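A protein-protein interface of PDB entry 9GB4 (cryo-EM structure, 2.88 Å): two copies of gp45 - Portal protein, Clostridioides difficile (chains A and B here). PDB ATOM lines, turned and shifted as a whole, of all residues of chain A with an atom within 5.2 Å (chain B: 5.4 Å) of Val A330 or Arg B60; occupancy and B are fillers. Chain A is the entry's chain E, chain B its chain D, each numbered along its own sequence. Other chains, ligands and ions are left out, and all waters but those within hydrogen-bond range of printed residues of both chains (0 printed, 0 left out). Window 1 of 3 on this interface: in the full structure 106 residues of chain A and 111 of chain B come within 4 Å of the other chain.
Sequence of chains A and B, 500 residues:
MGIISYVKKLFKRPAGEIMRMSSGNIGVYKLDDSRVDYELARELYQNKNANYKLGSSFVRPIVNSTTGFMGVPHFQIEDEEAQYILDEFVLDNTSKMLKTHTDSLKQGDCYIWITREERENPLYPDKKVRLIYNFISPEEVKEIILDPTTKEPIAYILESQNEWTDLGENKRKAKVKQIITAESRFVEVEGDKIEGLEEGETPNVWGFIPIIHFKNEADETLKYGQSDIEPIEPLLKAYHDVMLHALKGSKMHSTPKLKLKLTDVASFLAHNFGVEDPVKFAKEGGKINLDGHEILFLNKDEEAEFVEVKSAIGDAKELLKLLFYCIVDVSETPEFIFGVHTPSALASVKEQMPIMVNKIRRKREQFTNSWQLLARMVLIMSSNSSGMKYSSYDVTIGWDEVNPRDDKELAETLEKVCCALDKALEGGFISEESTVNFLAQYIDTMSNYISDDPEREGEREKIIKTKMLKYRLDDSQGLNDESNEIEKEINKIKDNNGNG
Val A330 touches two residues of chain B.
Of chain A, only Glu A217, Pro A231, Val A330, Glu A332 and Arg A362 come within 4 Å of Arg B60.
Of the printed residues of chain B, Cys A326 touches Ser B57.
Printed residues of chain B within 4 Å of Leu A235: Ser B57 (3.7 Å).
Of the printed residues of chain A, Asn B64 touches Glu A332 (2.5 Å) and Arg A362 (3.4 Å).
The nearest residue of chain B that does not touch Val A330 is Asn B47 (4.3 Å).
Printed residues of chain A that touch a printed residue of chain B: Glu A217, Pro A231, Leu A235, Cys A326, Asp A329, Val A330, Glu A332 and Arg A362.
Hydrophobic or aromatic side chains of chain A that line the printed part of chain B: Pro A231, Leu A235 and Val A330.
Of the 13 printed residues of chain B, 8 touch a printed residue of chain A.
Printed residues of chain B that touch a printed residue of chain A: Tyr B45, Gln B46, Asn B47, Ser B57, Phe B58, Arg B60, Pro B61 and Asn B64.
Hydrophobic or aromatic side chains of chain B within 4 Å of the printed part of chain A: Tyr B45, Phe B58 and Pro B61.
Among the printed residues, 17 pairs touch across the chains.
Among the printed residues, Asp or Glu carboxylates within 4 Å of a Lys or Arg side-chain nitrogen of the other chain: Glu A217 with Arg B60.
The backbone carbonyl oxygen (O) of Pro A231 lies within hydrogen-bond range of the side-chain amide nitrogen (ND2) of Asn B47 (2.8 Å).
OG of Ser B57 lies close to SG of Cys A326 (3.7 Å).
The side-chain carboxylate of Glu A217 lies within salt-bridge range of the guanidinium group of Arg B60 (3.0 Å).
The side-chain amide nitrogen of Asn B64 lies within hydrogen-bond range of the side-chain carboxylate of Glu A332 (2.5 Å).
The side-chain amide nitrogen (ND2) of Asn B64 sits close to the guanidinium group (NH2) of Arg A362, at 3.4 Å.
OE2 of Glu A332 lies close to O of Arg B60 (3.0 Å).
No position is printed for both chains.
Of the 17 pairs that touch across the chains among the printed residues, none has its exchanged pair printed and touching as well.
Among the printed residues, pairs that only touch across the chains: Glu A217 with Tyr B45 (3.9 Å), Pro A231 with Gln B46 (3.7 Å), Pro A231 with Arg B60 (3.9 Å), Leu A235 with Ser B57 (3.7 Å), Asp A329 with Ser B57 (3.9 Å), Asp A329 with Phe B58 (3.6 Å), Asp A329 with Pro B61 (3.3 Å), Val A330 with Ser B57 (3.5 Å), Val A330 with Arg B60 (3.5 Å), Glu A332 with Pro B61 (3.7 Å) and Arg A362 with Arg B60 (3.97 Å).
The side-chain amide oxygen (OD1) of Asn B64 lies within hydrogen-bond range of the side-chain hydroxyl (OH) of Tyr B45 (2.7 Å).
The side-chain amide oxygen (OE1) of Gln B46 sits at hydrogen-bond distance from the guanidinium group (NH1) of Arg B60, at 3.3 Å.
The side-chain amide oxygen of Asn B47 sits at hydrogen-bond distance from the side-chain hydroxyl of Ser B56.
O of Pro B61 is in hydrogen-bond range of OG of Ser B65 (2.7 Å).
The guanidinium group of Arg A362 is in salt-bridge range of the side-chain carboxylate of Glu A217, 3.4 Å away.
The side-chain carboxylate (OE1) of Glu A332 is in salt-bridge range of the guanidinium group (NH2) of Arg A362, at 3.96 Å.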
ATOM      1  N   GLU A 217      32.801  18.815   1.342  1.00  0.00           N
ATOM      2  CA  GLU A 217      31.957  18.435   0.210  1.00  0.00           C
ATOM      3  C   GLU A 217      32.668  18.709  -1.110  1.00  0.00           C
ATOM      4  O   GLU A 217      32.132  19.369  -2.002  1.00  0.00           O
ATOM      5  CB  GLU A 217      30.609  19.155   0.262  1.00  0.00           C
ATOM      6  CG  GLU A 217      29.746  18.782   1.451  1.00  0.00           C
ATOM      7  CD  GLU A 217      28.969  17.506   1.222  1.00  0.00           C
ATOM      8  OE1 GLU A 217      28.098  17.494   0.329  1.00  0.00           O
ATOM      9  OE2 GLU A 217      29.220  16.516   1.940  1.00  0.00           O
ATOM     10  N   PRO A 231      23.317  23.949   1.469  1.00  0.00           N
ATOM     11  CA  PRO A 231      22.063  23.226   1.209  1.00  0.00           C
ATOM     12  C   PRO A 231      20.876  23.742   2.002  1.00  0.00           C
ATOM     13  O   PRO A 231      19.757  23.757   1.477  1.00  0.00           O
ATOM     14  CB  PRO A 231      22.426  21.788   1.594  1.00  0.00           C
ATOM     15  CG  PRO A 231      23.858  21.697   1.326  1.00  0.00           C
ATOM     16  CD  PRO A 231      24.410  23.010   1.773  1.00  0.00           C
ATOM     17  N   ILE A 232      21.084  24.176   3.247  1.00  0.00           N
ATOM     18  CA  ILE A 232      19.970  24.588   4.098  1.00  0.00           C
ATOM     19  C   ILE A 232      19.657  26.078   4.009  1.00  0.00           C
ATOM     20  O   ILE A 232      18.601  26.499   4.500  1.00  0.00           O
ATOM     21  CB  ILE A 232      20.210  24.218   5.577  1.00  0.00           C
ATOM     22  CG1 ILE A 232      21.514  24.820   6.119  1.00  0.00           C
ATOM     23  CG2 ILE A 232      20.227  22.713   5.751  1.00  0.00           C
ATOM     24  CD1 ILE A 232      21.713  24.602   7.604  1.00  0.00           C
ATOM     25  N   LEU A 235      16.234  27.274   3.016  1.00  0.00           N
ATOM     26  CA  LEU A 235      15.293  26.878   4.052  1.00  0.00           C
ATOM     27  C   LEU A 235      15.440  27.730   5.303  1.00  0.00           C
ATOM     28  O   LEU A 235      14.436  28.055   5.942  1.00  0.00           O
ATOM     29  CB  LEU A 235      15.476  25.401   4.398  1.00  0.00           C
ATOM     30  CG  LEU A 235      15.248  24.421   3.250  1.00  0.00           C
ATOM     31  CD1 LEU A 235      15.847  23.076   3.590  1.00  0.00           C
ATOM     32  CD2 LEU A 235      13.769  24.286   2.943  1.00  0.00           C
ATOM     33  N   TYR A 325      11.338  20.076   9.180  1.00  0.00           N
ATOM     34  CA  TYR A 325      11.538  18.749   8.606  1.00  0.00           C
ATOM     35  C   TYR A 325      12.468  18.812   7.404  1.00  0.00           C
ATOM     36  O   TYR A 325      13.353  17.964   7.251  1.00  0.00           O
ATOM     37  CB  TYR A 325      10.198  18.138   8.190  1.00  0.00           C
ATOM     38  CG  TYR A 325       9.230  17.786   9.305  1.00  0.00           C
ATOM     39  CD1 TYR A 325       9.614  17.783  10.638  1.00  0.00           C
ATOM     40  CD2 TYR A 325       7.920  17.446   9.007  1.00  0.00           C
ATOM     41  CE1 TYR A 325       8.725  17.455  11.634  1.00  0.00           C
ATOM     42  CE2 TYR A 325       7.025  17.118   9.998  1.00  0.00           C
ATOM     43  CZ  TYR A 325       7.432  17.124  11.308  1.00  0.00           C
ATOM     44  OH  TYR A 325       6.538  16.798  12.299  1.00  0.00           O
ATOM     45  N   CYS A 326      12.278  19.807   6.538  1.00  0.00           N
ATOM     46  CA  CYS A 326      13.138  19.936   5.365  1.00  0.00           C
ATOM     47  C   CYS A 326      14.580  20.219   5.766  1.00  0.00           C
ATOM     48  O   CYS A 326      15.515  19.683   5.164  1.00  0.00           O
ATOM     49  CB  CYS A 326      12.611  21.038   4.448  1.00  0.00           C
ATOM     50  SG  CYS A 326      11.123  20.583   3.529  1.00  0.00           S
ATOM     51  N   ILE A 327      14.780  21.068   6.775  1.00  0.00           N
ATOM     52  CA  ILE A 327      16.130  21.374   7.237  1.00  0.00           C
ATOM     53  C   ILE A 327      16.789  20.129   7.809  1.00  0.00           C
ATOM     54  O   ILE A 327      17.972  19.867   7.564  1.00  0.00           O
ATOM     55  CB  ILE A 327      16.093  22.519   8.266  1.00  0.00           C
ATOM     56  CG1 ILE A 327      15.730  23.838   7.588  1.00  0.00           C
ATOM     57  CG2 ILE A 327      17.437  22.660   8.967  1.00  0.00           C
ATOM     58  CD1 ILE A 327      15.104  24.845   8.518  1.00  0.00           C
ATOM     59  N   VAL A 328      16.043  19.346   8.591  1.00  0.00           N
ATOM     60  CA  VAL A 328      16.602  18.126   9.165  1.00  0.00           C
ATOM     61  C   VAL A 328      16.939  17.129   8.063  1.00  0.00           C
ATOM     62  O   VAL A 328      17.959  16.436   8.126  1.00  0.00           O
ATOM     63  CB  VAL A 328      15.630  17.522  10.195  1.00  0.00           C
ATOM     64  CG1 VAL A 328      16.099  16.146  10.632  1.00  0.00           C
ATOM     65  CG2 VAL A 328      15.497  18.426  11.405  1.00  0.00           C
ATOM     66  N   ASP A 329      16.084  17.034   7.042  1.00  0.00           N
ATOM     67  CA  ASP A 329      16.351  16.135   5.925  1.00  0.00           C
ATOM     68  C   ASP A 329      17.619  16.545   5.187  1.00  0.00           C
ATOM     69  O   ASP A 329      18.491  15.715   4.915  1.00  0.00           O
ATOM     70  CB  ASP A 329      15.161  16.124   4.965  1.00  0.00           C
ATOM     71  CG  ASP A 329      13.930  15.480   5.563  1.00  0.00           C
ATOM     72  OD1 ASP A 329      14.063  14.735   6.554  1.00  0.00           O
ATOM     73  OD2 ASP A 329      12.825  15.721   5.036  1.00  0.00           O
ATOM     74  N   VAL A 330      17.734  17.834   4.860  1.00  0.00           N
ATOM     75  CA  VAL A 330      18.862  18.313   4.064  1.00  0.00           C
ATOM     76  C   VAL A 330      20.174  18.077   4.797  1.00  0.00           C
ATOM     77  O   VAL A 330      21.127  17.528   4.235  1.00  0.00           O
ATOM     78  CB  VAL A 330      18.668  19.803   3.727  1.00  0.00           C
ATOM     79  CG1 VAL A 330      19.934  20.409   3.191  1.00  0.00           C
ATOM     80  CG2 VAL A 330      17.584  19.969   2.713  1.00  0.00           C
ATOM     81  N   SER A 331      20.245  18.490   6.057  1.00  0.00           N
ATOM     82  CA  SER A 331      21.458  18.319   6.838  1.00  0.00           C
ATOM     83  C   SER A 331      21.712  16.872   7.232  1.00  0.00           C
ATOM     84  O   SER A 331      22.832  16.550   7.639  1.00  0.00           O
ATOM     85  CB  SER A 331      21.387  19.178   8.096  1.00  0.00           C
ATOM     86  OG  SER A 331      20.285  18.800   8.899  1.00  0.00           O
ATOM     87  N   GLU A 332      20.706  16.003   7.136  1.00  0.00           N
ATOM     88  CA  GLU A 332      20.826  14.595   7.501  1.00  0.00           C
ATOM     89  C   GLU A 332      21.175  14.415   8.970  1.00  0.00           C
ATOM     90  O   GLU A 332      21.748  13.392   9.353  1.00  0.00           O
ATOM     91  CB  GLU A 332      21.863  13.881   6.630  1.00  0.00           C
ATOM     92  CG  GLU A 332      21.655  14.066   5.146  1.00  0.00           C
ATOM     93  CD  GLU A 332      22.772  13.472   4.333  1.00  0.00           C
ATOM     94  OE1 GLU A 332      23.648  12.802   4.916  1.00  0.00           O
ATOM     95  OE2 GLU A 332      22.785  13.699   3.107  1.00  0.00           O
ATOM     96  N   ARG A 362      30.457   8.719   6.081  1.00  0.00           N
ATOM     97  CA  ARG A 362      30.492   9.413   4.799  1.00  0.00           C
ATOM     98  C   ARG A 362      31.315  10.692   4.892  1.00  0.00           C
ATOM     99  O   ARG A 362      32.061  11.033   3.967  1.00  0.00           O
ATOM    100  CB  ARG A 362      29.072   9.720   4.330  1.00  0.00           C
ATOM    101  CG  ARG A 362      28.986  10.095   2.858  1.00  0.00           C
ATOM    102  CD  ARG A 362      27.590  10.533   2.469  1.00  0.00           C
ATOM    103  NE  ARG A 362      27.186  11.746   3.168  1.00  0.00           N
ATOM    104  CZ  ARG A 362      27.635  12.965   2.896  1.00  0.00           C
ATOM    105  NH1 ARG A 362      28.518  13.183   1.933  1.00  0.00           N
ATOM    106  NH2 ARG A 362      27.187  13.993   3.608  1.00  0.00           N
ATOM    107  N   TYR B  45      20.811  18.087  -5.910  1.00  0.00           N
ATOM    108  CA  TYR B  45      21.503  17.516  -4.760  1.00  0.00           C
ATOM    109  C   TYR B  45      21.932  18.608  -3.792  1.00  0.00           C
ATOM    110  O   TYR B  45      21.766  18.475  -2.576  1.00  0.00           O
ATOM    111  CB  TYR B  45      22.706  16.702  -5.226  1.00  0.00           C
ATOM    112  CG  TYR B  45      23.546  16.138  -4.104  1.00  0.00           C
ATOM    113  CD1 TYR B  45      24.685  16.793  -3.663  1.00  0.00           C
ATOM    114  CD2 TYR B  45      23.200  14.945  -3.490  1.00  0.00           C
ATOM    115  CE1 TYR B  45      25.452  16.276  -2.642  1.00  0.00           C
ATOM    116  CE2 TYR B  45      23.961  14.422  -2.471  1.00  0.00           C
ATOM    117  CZ  TYR B  45      25.085  15.091  -2.051  1.00  0.00           C
ATOM    118  OH  TYR B  45      25.845  14.570  -1.032  1.00  0.00           O
ATOM    119  N   GLN B  46      22.470  19.704  -4.314  1.00  0.00           N
ATOM    120  CA  GLN B  46      22.939  20.804  -3.483  1.00  0.00           C
ATOM    121  C   GLN B  46      21.829  21.789  -3.122  1.00  0.00           C
ATOM    122  O   GLN B  46      22.105  22.782  -2.445  1.00  0.00           O
ATOM    123  CB  GLN B  46      24.082  21.535  -4.195  1.00  0.00           C
ATOM    124  CG  GLN B  46      25.050  22.273  -3.278  1.00  0.00           C
ATOM    125  CD  GLN B  46      25.832  21.342  -2.371  1.00  0.00           C
ATOM    126  OE1 GLN B  46      25.836  20.127  -2.568  1.00  0.00           O
ATOM    127  NE2 GLN B  46      26.491  21.906  -1.367  1.00  0.00           N
ATOM    128  N   ASN B  47      20.592  21.548  -3.560  1.00  0.00           N
ATOM    129  CA  ASN B  47      19.443  22.360  -3.162  1.00  0.00           C
ATOM    130  C   ASN B  47      19.542  23.783  -3.705  1.00  0.00           C
ATOM    131  O   ASN B  47      19.117  24.739  -3.053  1.00  0.00           O
ATOM    132  CB  ASN B  47      19.288  22.372  -1.637  1.00  0.00           C
ATOM    133  CG  ASN B  47      17.841  22.389  -1.191  1.00  0.00           C
ATOM    134  OD1 ASN B  47      17.002  21.676  -1.734  1.00  0.00           O
ATOM    135  ND2 ASN B  47      17.543  23.199  -0.185  1.00  0.00           N
ATOM    136  N   SER B  56      13.458  19.803  -3.162  1.00  0.00           N
ATOM    137  CA  SER B  56      14.663  18.993  -3.297  1.00  0.00           C
ATOM    138  C   SER B  56      15.371  18.741  -1.972  1.00  0.00           C
ATOM    139  O   SER B  56      16.543  18.354  -1.980  1.00  0.00           O
ATOM    140  CB  SER B  56      15.627  19.662  -4.279  1.00  0.00           C
ATOM    141  OG  SER B  56      15.834  21.019  -3.942  1.00  0.00           O
ATOM    142  N   SER B  57      14.702  18.950  -0.838  1.00  0.00           N
ATOM    143  CA  SER B  57      15.292  18.599   0.446  1.00  0.00           C
ATOM    144  C   SER B  57      15.544  17.105   0.570  1.00  0.00           C
ATOM    145  O   SER B  57      16.428  16.685   1.322  1.00  0.00           O
ATOM    146  CB  SER B  57      14.376  19.072   1.574  1.00  0.00           C
ATOM    147  OG  SER B  57      14.236  20.479   1.552  1.00  0.00           O
ATOM    148  N   PHE B  58      14.781  16.288  -0.155  1.00  0.00           N
ATOM    149  CA  PHE B  58      14.856  14.843  -0.001  1.00  0.00           C
ATOM    150  C   PHE B  58      16.020  14.214  -0.754  1.00  0.00           C
ATOM    151  O   PHE B  58      16.348  13.055  -0.488  1.00  0.00           O
ATOM    152  CB  PHE B  58      13.549  14.214  -0.478  1.00  0.00           C
ATOM    153  CG  PHE B  58      12.347  14.680   0.281  1.00  0.00           C
ATOM    154  CD1 PHE B  58      12.055  14.162   1.525  1.00  0.00           C
ATOM    155  CD2 PHE B  58      11.514  15.647  -0.246  1.00  0.00           C
ATOM    156  CE1 PHE B  58      10.952  14.593   2.226  1.00  0.00           C
ATOM    157  CE2 PHE B  58      10.412  16.081   0.453  1.00  0.00           C
ATOM    158  CZ  PHE B  58      10.131  15.553   1.689  1.00  0.00           C
ATOM    159  N   VAL B  59      16.652  14.938  -1.679  1.00  0.00           N
ATOM    160  CA  VAL B  59      17.676  14.328  -2.523  1.00  0.00           C
ATOM    161  C   VAL B  59      18.891  13.932  -1.696  1.00  0.00           C
ATOM    162  O   VAL B  59      19.419  12.823  -1.838  1.00  0.00           O
ATOM    163  CB  VAL B  59      18.070  15.279  -3.663  1.00  0.00           C
ATOM    164  CG1 VAL B  59      19.195  14.665  -4.482  1.00  0.00           C
ATOM    165  CG2 VAL B  59      16.864  15.579  -4.532  1.00  0.00           C
ATOM    166  N   ARG B  60      19.364  14.834  -0.840  1.00  0.00           N
ATOM    167  CA  ARG B  60      20.574  14.558  -0.066  1.00  0.00           C
ATOM    168  C   ARG B  60      20.442  13.346   0.842  1.00  0.00           C
ATOM    169  O   ARG B  60      21.328  12.476   0.793  1.00  0.00           O
ATOM    170  CB  ARG B  60      20.960  15.795   0.745  1.00  0.00           C
ATOM    171  CG  ARG B  60      21.552  16.901  -0.090  1.00  0.00           C
ATOM    172  CD  ARG B  60      22.178  17.980   0.762  1.00  0.00           C
ATOM    173  NE  ARG B  60      23.345  17.510   1.499  1.00  0.00           N
ATOM    174  CZ  ARG B  60      24.609  17.647   1.117  1.00  0.00           C
ATOM    175  NH1 ARG B  60      24.937  18.218  -0.032  1.00  0.00           N
ATOM    176  NH2 ARG B  60      25.575  17.193   1.909  1.00  0.00           N
ATOM    177  N   PRO B  61      19.418  13.224   1.696  1.00  0.00           N
ATOM    178  CA  PRO B  61      19.349  12.034   2.558  1.00  0.00           C
ATOM    179  C   PRO B  61      19.265  10.733   1.787  1.00  0.00           C
ATOM    180  O   PRO B  61      19.934   9.770   2.168  1.00  0.00           O
ATOM    181  CB  PRO B  61      18.091  12.277   3.405  1.00  0.00           C
ATOM    182  CG  PRO B  61      17.344  13.332   2.715  1.00  0.00           C
ATOM    183  CD  PRO B  61      18.350  14.180   2.029  1.00  0.00           C
ATOM    184  N   ILE B  62      18.525  10.697   0.680  1.00  0.00           N
ATOM    185  CA  ILE B  62      18.401   9.470  -0.102  1.00  0.00           C
ATOM    186  C   ILE B  62      19.762   9.036  -0.631  1.00  0.00           C
ATOM    187  O   ILE B  62      20.252   7.939  -0.323  1.00  0.00           O
ATOM    188  CB  ILE B  62      17.395   9.679  -1.250  1.00  0.00           C
ATOM    189  CG1 ILE B  62      15.973   9.804  -0.701  1.00  0.00           C
ATOM    190  CG2 ILE B  62      17.473   8.540  -2.261  1.00  0.00           C
ATOM    191  CD1 ILE B  62      15.010  10.501  -1.636  1.00  0.00           C
ATOM    192  N   VAL B  63      20.396   9.902  -1.424  1.00  0.00           N
ATOM    193  CA  VAL B  63      21.653   9.556  -2.075  1.00  0.00           C
ATOM    194  C   VAL B  63      22.731   9.275  -1.040  1.00  0.00           C
ATOM    195  O   VAL B  63      23.473   8.294  -1.150  1.00  0.00           O
ATOM    196  CB  VAL B  63      22.074  10.685  -3.034  1.00  0.00           C
ATOM    197  CG1 VAL B  63      23.502  10.476  -3.525  1.00  0.00           C
ATOM    198  CG2 VAL B  63      21.102  10.777  -4.199  1.00  0.00           C
ATOM    199  N   ASN B  64      22.830  10.117  -0.013  1.00  0.00           N
ATOM    200  CA  ASN B  64      23.919   9.959   0.938  1.00  0.00           C
ATOM    201  C   ASN B  64      23.713   8.768   1.862  1.00  0.00           C
ATOM    202  O   ASN B  64      24.691   8.112   2.221  1.00  0.00           O
ATOM    203  CB  ASN B  64      24.099  11.239   1.747  1.00  0.00           C
ATOM    204  CG  ASN B  64      24.699  12.365   0.924  1.00  0.00           C
ATOM    205  OD1 ASN B  64      25.239  12.138  -0.156  1.00  0.00           O
ATOM    206  ND2 ASN B  64      24.623  13.583   1.439  1.00  0.00           N
ATOM    207  N   SER B  65      22.477   8.450   2.251  1.00  0.00           N
ATOM    208  CA  SER B  65      22.251   7.239   3.028  1.00  0.00           C
ATOM    209  C   SER B  65      22.581   6.005   2.204  1.00  0.00           C
ATOM    210  O   SER B  65      23.248   5.080   2.687  1.00  0.00           O
ATOM    211  CB  SER B  65      20.805   7.190   3.514  1.00  0.00           C
ATOM    212  OG  SER B  65      19.908   7.111   2.423  1.00  0.00           O
